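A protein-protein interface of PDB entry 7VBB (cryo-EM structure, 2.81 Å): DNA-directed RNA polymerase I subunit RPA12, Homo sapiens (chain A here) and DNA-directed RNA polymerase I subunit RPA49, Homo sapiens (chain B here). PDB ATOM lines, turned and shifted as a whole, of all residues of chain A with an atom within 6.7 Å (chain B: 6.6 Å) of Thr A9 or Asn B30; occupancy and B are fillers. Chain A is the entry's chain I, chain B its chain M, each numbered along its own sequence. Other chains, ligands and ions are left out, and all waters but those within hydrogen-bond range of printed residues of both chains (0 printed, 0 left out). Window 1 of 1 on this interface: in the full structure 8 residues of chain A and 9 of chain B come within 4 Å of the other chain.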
ATOM      1  N   ALA A   7     -10.517  18.406 -29.012  1.00  0.00           N
ATOM      2  CA  ALA A   7      -9.609  19.493 -29.425  1.00  0.00           C
ATOM      3  C   ALA A   7     -10.234  20.344 -30.532  1.00  0.00           C
ATOM      4  O   ALA A   7     -10.289  21.559 -30.327  1.00  0.00           O
ATOM      5  CB  ALA A   7      -8.253  18.938 -29.727  1.00  0.00           C
ATOM      6  N   ASN A   8     -10.752  19.754 -31.612  1.00  0.00           N
ATOM      7  CA  ASN A   8     -11.473  20.548 -32.648  1.00  0.00           C
ATOM      8  C   ASN A   8     -12.985  20.476 -32.425  1.00  0.00           C
ATOM      9  O   ASN A   8     -13.712  20.359 -33.419  1.00  0.00           O
ATOM     10  CB  ASN A   8     -11.106  20.125 -34.068  1.00  0.00           C
ATOM     11  CG  ASN A   8     -10.181  21.105 -34.758  1.00  0.00           C
ATOM     12  OD1 ASN A   8      -9.849  22.149 -34.203  1.00  0.00           O
ATOM     13  ND2 ASN A   8      -9.766  20.777 -35.972  1.00  0.00           N
ATOM     14  N   THR A   9     -13.429  20.574 -31.172  1.00  0.00           N
ATOM     15  CA  THR A   9     -14.844  20.561 -30.832  1.00  0.00           C
ATOM     16  C   THR A   9     -15.264  21.953 -30.375  1.00  0.00           C
ATOM     17  O   THR A   9     -14.563  22.615 -29.604  1.00  0.00           O
ATOM     18  CB  THR A   9     -15.130  19.523 -29.749  1.00  0.00           C
ATOM     19  OG1 THR A   9     -16.540  19.462 -29.502  1.00  0.00           O
ATOM     20  CG2 THR A   9     -14.420  19.883 -28.473  1.00  0.00           C
ATOM     21  N   CYS A  10     -16.424  22.398 -30.850  1.00  0.00           N
ATOM     22  CA  CYS A  10     -16.731  23.819 -30.937  1.00  0.00           C
ATOM     23  C   CYS A  10     -17.705  24.272 -29.858  1.00  0.00           C
ATOM     24  O   CYS A  10     -18.890  23.923 -29.897  1.00  0.00           O
ATOM     25  CB  CYS A  10     -17.299  24.162 -32.315  1.00  0.00           C
ATOM     26  SG  CYS A  10     -16.125  23.977 -33.672  1.00  0.00           S
ATOM     27  N   SER A  11     -17.194  25.036 -28.894  1.00  0.00           N
ATOM     28  CA  SER A  11     -17.974  26.031 -28.164  1.00  0.00           C
ATOM     29  C   SER A  11     -18.991  25.466 -27.179  1.00  0.00           C
ATOM     30  O   SER A  11     -19.609  26.227 -26.430  1.00  0.00           O
ATOM     31  CB  SER A  11     -18.692  26.946 -29.159  1.00  0.00           C
ATOM     32  OG  SER A  11     -17.784  27.463 -30.114  1.00  0.00           O
ATOM     33  N   SER A  12     -19.178  24.151 -27.155  1.00  0.00           N
ATOM     34  CA  SER A  12     -20.122  23.543 -26.230  1.00  0.00           C
ATOM     35  C   SER A  12     -19.606  22.245 -25.626  1.00  0.00           C
ATOM     36  O   SER A  12     -20.354  21.565 -24.919  1.00  0.00           O
ATOM     37  CB  SER A  12     -21.462  23.302 -26.924  1.00  0.00           C
ATOM     38  OG  SER A  12     -22.470  22.997 -25.978  1.00  0.00           O
ATOM     39  N   PHE A  13     -18.348  21.895 -25.877  1.00  0.00           N
ATOM     40  CA  PHE A  13     -17.768  20.663 -25.372  1.00  0.00           C
ATOM     41  C   PHE A  13     -16.332  20.922 -24.934  1.00  0.00           C
ATOM     42  O   PHE A  13     -15.634  21.762 -25.507  1.00  0.00           O
ATOM     43  CB  PHE A  13     -17.856  19.559 -26.434  1.00  0.00           C
ATOM     44  CG  PHE A  13     -19.264  19.292 -26.899  1.00  0.00           C
ATOM     45  CD1 PHE A  13     -20.138  18.562 -26.118  1.00  0.00           C
ATOM     46  CD2 PHE A  13     -19.721  19.799 -28.102  1.00  0.00           C
ATOM     47  CE1 PHE A  13     -21.432  18.330 -26.533  1.00  0.00           C
ATOM     48  CE2 PHE A  13     -21.014  19.568 -28.518  1.00  0.00           C
ATOM     49  CZ  PHE A  13     -21.869  18.835 -27.732  1.00  0.00           C
ATOM     50  N   GLN A  14     -16.293  19.681 -24.292  1.00  0.00           N
ATOM     51  CA  GLN A  14     -15.082  19.910 -23.506  1.00  0.00           C
ATOM     52  C   GLN A  14     -13.824  19.918 -24.371  1.00  0.00           C
ATOM     53  O   GLN A  14     -12.860  20.625 -24.062  1.00  0.00           O
ATOM     54  CB  GLN A  14     -14.985  18.861 -22.397  1.00  0.00           C
ATOM     55  CG  GLN A  14     -15.543  19.344 -21.063  1.00  0.00           C
ATOM     56  CD  GLN A  14     -16.034  18.218 -20.173  1.00  0.00           C
ATOM     57  OE1 GLN A  14     -16.458  17.170 -20.654  1.00  0.00           O
ATOM     58  NE2 GLN A  14     -15.986  18.434 -18.868  1.00  0.00           N
ATOM     59  N   SER A  15     -13.804  19.299 -25.539  1.00  0.00           N
ATOM     60  CA  SER A  15     -12.547  19.272 -26.347  1.00  0.00           C
ATOM     61  C   SER A  15     -11.588  18.238 -25.835  1.00  0.00           C
ATOM     62  O   SER A  15     -11.332  17.257 -26.534  1.00  0.00           O
ATOM     63  CB  SER A  15     -11.835  20.589 -26.511  1.00  0.00           C
ATOM     64  OG  SER A  15     -11.737  20.988 -27.867  1.00  0.00           O
ATOM     65  N   ASP A  16     -10.973  18.539 -24.714  1.00  0.00           N
ATOM     66  CA  ASP A  16     -10.149  17.458 -24.169  1.00  0.00           C
ATOM     67  C   ASP A  16     -11.092  16.342 -23.726  1.00  0.00           C
ATOM     68  O   ASP A  16     -11.060  15.273 -24.316  1.00  0.00           O
ATOM     69  CB  ASP A  16      -9.300  18.018 -23.033  1.00  0.00           C
ATOM     70  CG  ASP A  16      -8.106  18.798 -23.550  1.00  0.00           C
ATOM     71  OD1 ASP A  16      -8.247  19.457 -24.599  1.00  0.00           O
ATOM     72  OD2 ASP A  16      -7.039  18.715 -22.920  1.00  0.00           O
ATOM     73  N   LEU A  17     -12.092  16.659 -22.932  1.00  0.00           N
ATOM     74  CA  LEU A  17     -12.890  15.563 -22.336  1.00  0.00           C
ATOM     75  C   LEU A  17     -13.944  15.136 -23.319  1.00  0.00           C
ATOM     76  O   LEU A  17     -13.618  14.901 -24.481  1.00  0.00           O
ATOM     77  CB  LEU A  17     -13.430  16.122 -21.024  1.00  0.00           C
ATOM     78  CG  LEU A  17     -12.279  16.890 -20.367  1.00  0.00           C
ATOM     79  CD1 LEU A  17     -12.630  18.238 -19.773  1.00  0.00           C
ATOM     80  CD2 LEU A  17     -11.397  16.029 -19.477  1.00  0.00           C
ATOM     81  N   ASP A  18     -15.182  15.065 -22.863  1.00  0.00           N
ATOM     82  CA  ASP A  18     -16.096  14.612 -23.935  1.00  0.00           C
ATOM     83  C   ASP A  18     -17.433  15.303 -23.822  1.00  0.00           C
ATOM     84  O   ASP A  18     -17.902  15.769 -24.858  1.00  0.00           O
ATOM     85  CB  ASP A  18     -16.343  13.110 -23.818  1.00  0.00           C
ATOM     86  CG  ASP A  18     -16.708  12.603 -22.431  1.00  0.00           C
ATOM     87  OD1 ASP A  18     -16.202  13.176 -21.447  1.00  0.00           O
ATOM     88  OD2 ASP A  18     -17.496  11.639 -22.351  1.00  0.00           O
ATOM     89  N   PHE A  19     -18.014  15.291 -22.612  1.00  0.00           N
ATOM     90  CA  PHE A  19     -19.356  15.829 -22.449  1.00  0.00           C
ATOM     91  C   PHE A  19     -19.453  17.247 -23.010  1.00  0.00           C
ATOM     92  O   PHE A  19     -18.483  17.822 -23.510  1.00  0.00           O
ATOM     93  CB  PHE A  19     -19.751  15.800 -20.974  1.00  0.00           C
ATOM     94  CG  PHE A  19     -19.221  14.602 -20.236  1.00  0.00           C
ATOM     95  CD1 PHE A  19     -19.794  13.354 -20.418  1.00  0.00           C
ATOM     96  CD2 PHE A  19     -18.139  14.719 -19.381  1.00  0.00           C
ATOM     97  CE1 PHE A  19     -19.308  12.247 -19.745  1.00  0.00           C
ATOM     98  CE2 PHE A  19     -17.649  13.616 -18.707  1.00  0.00           C
ATOM     99  CZ  PHE A  19     -18.233  12.379 -18.890  1.00  0.00           C
ATOM    100  N   GLN B  27      -7.999   7.119 -34.187  1.00  0.00           N
ATOM    101  CA  GLN B  27      -9.118   8.028 -34.401  1.00  0.00           C
ATOM    102  C   GLN B  27      -9.736   8.464 -33.076  1.00  0.00           C
ATOM    103  O   GLN B  27     -10.063   7.628 -32.233  1.00  0.00           O
ATOM    104  CB  GLN B  27     -10.183   7.370 -35.284  1.00  0.00           C
ATOM    105  CG  GLN B  27     -11.332   8.296 -35.656  1.00  0.00           C
ATOM    106  CD  GLN B  27     -12.360   7.628 -36.551  1.00  0.00           C
ATOM    107  OE1 GLN B  27     -12.627   6.430 -36.423  1.00  0.00           O
ATOM    108  NE2 GLN B  27     -12.940   8.398 -37.464  1.00  0.00           N
ATOM    109  N   PHE B  28      -9.924   9.750 -32.889  1.00  0.00           N
ATOM    110  CA  PHE B  28     -10.464  10.294 -31.648  1.00  0.00           C
ATOM    111  C   PHE B  28     -11.970  10.495 -31.754  1.00  0.00           C
ATOM    112  O   PHE B  28     -12.457  11.070 -32.730  1.00  0.00           O
ATOM    113  CB  PHE B  28      -9.778  11.618 -31.299  1.00  0.00           C
ATOM    114  CG  PHE B  28      -8.334  11.470 -30.907  1.00  0.00           C
ATOM    115  CD1 PHE B  28      -7.340  11.446 -31.879  1.00  0.00           C
ATOM    116  CD2 PHE B  28      -7.967  11.357 -29.572  1.00  0.00           C
ATOM    117  CE1 PHE B  28      -6.000  11.311 -31.522  1.00  0.00           C
ATOM    118  CE2 PHE B  28      -6.629  11.221 -29.208  1.00  0.00           C
ATOM    119  CZ  PHE B  28      -5.648  11.199 -30.189  1.00  0.00           C
ATOM    120  N   SER B  29     -12.745  10.020 -30.857  1.00  0.00           N
ATOM    121  CA  SER B  29     -14.202  10.071 -30.878  1.00  0.00           C
ATOM    122  C   SER B  29     -14.708  11.506 -30.778  1.00  0.00           C
ATOM    123  O   SER B  29     -15.812  11.812 -31.231  1.00  0.00           O
ATOM    124  CB  SER B  29     -14.784   9.236 -29.736  1.00  0.00           C
ATOM    125  OG  SER B  29     -14.292   9.683 -28.485  1.00  0.00           O
ATOM    126  N   ASN B  30     -13.930  12.437 -30.202  1.00  0.00           N
ATOM    127  CA  ASN B  30     -14.406  13.796 -29.969  1.00  0.00           C
ATOM    128  C   ASN B  30     -13.786  14.785 -30.953  1.00  0.00           C
ATOM    129  O   ASN B  30     -13.684  15.977 -30.661  1.00  0.00           O
ATOM    130  CB  ASN B  30     -14.116  14.228 -28.529  1.00  0.00           C
ATOM    131  CG  ASN B  30     -14.871  13.400 -27.510  1.00  0.00           C
ATOM    132  OD1 ASN B  30     -15.982  12.932 -27.771  1.00  0.00           O
ATOM    133  ND2 ASN B  30     -14.276  13.215 -26.337  1.00  0.00           N
ATOM    134  N   GLY B  31     -13.311  14.265 -32.051  1.00  0.00           N
ATOM    135  CA  GLY B  31     -12.760  15.178 -33.039  1.00  0.00           C
ATOM    136  C   GLY B  31     -11.261  15.028 -33.217  1.00  0.00           C
ATOM    137  O   GLY B  31     -10.729  13.919 -33.139  1.00  0.00           O
ATOM    138  N   LYS B  32     -10.616  16.163 -33.704  1.00  0.00           N
ATOM    139  CA  LYS B  32      -9.192  16.197 -34.025  1.00  0.00           C
ATOM    140  C   LYS B  32      -8.389  16.839 -32.896  1.00  0.00           C
ATOM    141  O   LYS B  32      -8.892  17.719 -32.193  1.00  0.00           O
ATOM    142  CB  LYS B  32      -8.953  16.952 -35.333  1.00  0.00           C
ATOM    143  CG  LYS B  32      -7.515  16.898 -35.826  1.00  0.00           C
ATOM    144  CD  LYS B  32      -7.350  17.627 -37.152  1.00  0.00           C
ATOM    145  CE  LYS B  32      -5.900  17.627 -37.617  1.00  0.00           C
ATOM    146  NZ  LYS B  32      -5.730  18.367 -38.903  1.00  0.00           N
ATOM    147  N   GLN B  34      -5.834  19.146 -31.608  1.00  0.00           N
ATOM    148  CA  GLN B  34      -5.233  20.407 -32.034  1.00  0.00           C
ATOM    149  C   GLN B  34      -3.712  20.344 -31.966  1.00  0.00           C
ATOM    150  O   GLN B  34      -3.021  20.890 -32.827  1.00  0.00           O
ATOM    151  CB  GLN B  34      -5.751  21.566 -31.181  1.00  0.00           C
ATOM    152  CG  GLN B  34      -7.200  21.936 -31.461  1.00  0.00           C
ATOM    153  CD  GLN B  34      -7.641  23.186 -30.719  1.00  0.00           C
ATOM    154  OE1 GLN B  34      -6.914  23.709 -29.868  1.00  0.00           O
ATOM    155  NE2 GLN B  34      -8.837  23.672 -31.035  1.00  0.00           N
ATOM    156  N   TYR B  69      -6.560   9.280 -23.094  1.00  0.00           N
ATOM    157  CA  TYR B  69      -7.386   8.573 -24.066  1.00  0.00           C
ATOM    158  C   TYR B  69      -6.998   7.100 -24.143  1.00  0.00           C
ATOM    159  O   TYR B  69      -5.822   6.756 -24.016  1.00  0.00           O
ATOM    160  CB  TYR B  69      -7.263   9.217 -25.450  1.00  0.00           C
ATOM    161  CG  TYR B  69      -7.758  10.642 -25.500  1.00  0.00           C
ATOM    162  CD1 TYR B  69      -6.947  11.693 -25.085  1.00  0.00           C
ATOM    163  CD2 TYR B  69      -9.035  10.941 -25.967  1.00  0.00           C
ATOM    164  CE1 TYR B  69      -7.397  13.009 -25.131  1.00  0.00           C
ATOM    165  CE2 TYR B  69      -9.495  12.252 -26.019  1.00  0.00           C
ATOM    166  CZ  TYR B  69      -8.670  13.279 -25.598  1.00  0.00           C
ATOM    167  OH  TYR B  69      -9.120  14.578 -25.647  1.00  0.00           O
ATOM    168  N   MET B 109     -10.017   6.219 -30.137  1.00  0.00           N
ATOM    169  CA  MET B 109      -9.576   6.753 -28.852  1.00  0.00           C
ATOM    170  C   MET B 109     -10.729   7.428 -28.116  1.00  0.00           C
ATOM    171  O   MET B 109     -11.408   8.291 -28.679  1.00  0.00           O
ATOM    172  CB  MET B 109      -8.427   7.744 -29.046  1.00  0.00           C
ATOM    173  CG  MET B 109      -7.235   7.163 -29.791  1.00  0.00           C
ATOM    174  SD  MET B 109      -6.477   5.746 -28.903  1.00  0.00           S
ATOM    175  CE  MET B 109      -5.726   6.612 -27.499  1.00  0.00           C
ATOM    176  N   GLN B 110     -10.622   7.283 -26.754  1.00  0.00           N
ATOM    177  CA  GLN B 110     -11.647   7.812 -25.794  1.00  0.00           C
ATOM    178  C   GLN B 110     -11.067   8.289 -24.434  1.00  0.00           C
ATOM    179  O   GLN B 110     -10.215   7.597 -23.916  1.00  0.00           O
ATOM    180  CB  GLN B 110     -12.493   6.629 -25.331  1.00  0.00           C
ATOM    181  CG  GLN B 110     -13.768   6.425 -26.125  1.00  0.00           C
ATOM    182  CD  GLN B 110     -14.964   6.838 -25.305  1.00  0.00           C
ATOM    183  OE1 GLN B 110     -14.993   6.658 -24.090  1.00  0.00           O
ATOM    184  NE2 GLN B 110     -15.959   7.399 -25.972  1.00  0.00           N
ATOM    185  N   PRO B 111     -11.609   9.328 -23.738  1.00  0.00           N
ATOM    186  CA  PRO B 111     -11.121   9.879 -22.411  1.00  0.00           C
ATOM    187  C   PRO B 111     -11.095   9.050 -21.109  1.00  0.00           C
ATOM    188  O   PRO B 111     -12.034   8.303 -20.911  1.00  0.00           O
ATOM    189  CB  PRO B 111     -12.084  11.029 -22.108  1.00  0.00           C
ATOM    190  CG  PRO B 111     -12.566  11.446 -23.467  1.00  0.00           C
ATOM    191  CD  PRO B 111     -12.738  10.138 -24.207  1.00  0.00           C
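The side-chain amide oxygen (OE1) of Gln A14 lies within hydrogen-bond range of the backbone NH (N) of Asp A18 (3.3 Å).
The backbone NH (N) of Ala A7 is in hydrogen-bond range of the backbone carbonyl oxygen (O) of Ser A15 (2.9 Å).
Among the printed residues, pairs that only touch across the chains: Ala A7 with Lys B32, Asn A8 with Gln B34, Thr A9 with Asn B30, Ser A15 with Tyr B69, Leu A17 with Pro B111 and Asp A18 with Asn B30.
Of the printed residues of chain B, Asn A8 touches Lys B32 and Gln B34.
Thr A9 touches just one residue of chain B: Asn B30.
Ser A12 touches none of the printed residues of chain B.
Phe A13 touches none of the printed residues of chain B.
Of the printed residues of chain B, Ser A15 touches Tyr B69 (3.6 Å).
Asn B30 touches three residues of chain A.
Printed residues of chain A within 4 Å of Tyr B69: Ser A15 and Asp A16.
Of the printed residues of chain A, Pro B111 touches Leu A17 (3.8 Å).
The nearest printed residue of chain A that does not touch Asn B30 is Ala A7 (4.3 Å).
The nearest printed residue of chain B that does not touch Asn A8 is Asn B30 (4.9 Å).
Hydrophobic or aromatic side chains of chain B that line the printed part of chain A: Tyr B69 and Pro B111.
Among the printed residues, 10 pairs touch across the chains.
N of Asn A8 lies within hydrogen-bond range of O of Lys B32 (2.8 Å).
O of Asp A16 is in hydrogen-bond range of OH of Tyr B69.
The backbone carbonyl oxygen of Leu A17 sits at hydrogen-bond distance from the side-chain amide nitrogen of Asn B30 (2.6 Å).
NE2 of Gln B34 is in hydrogen-bond range of O of Ala A7, 2.7 Å away.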
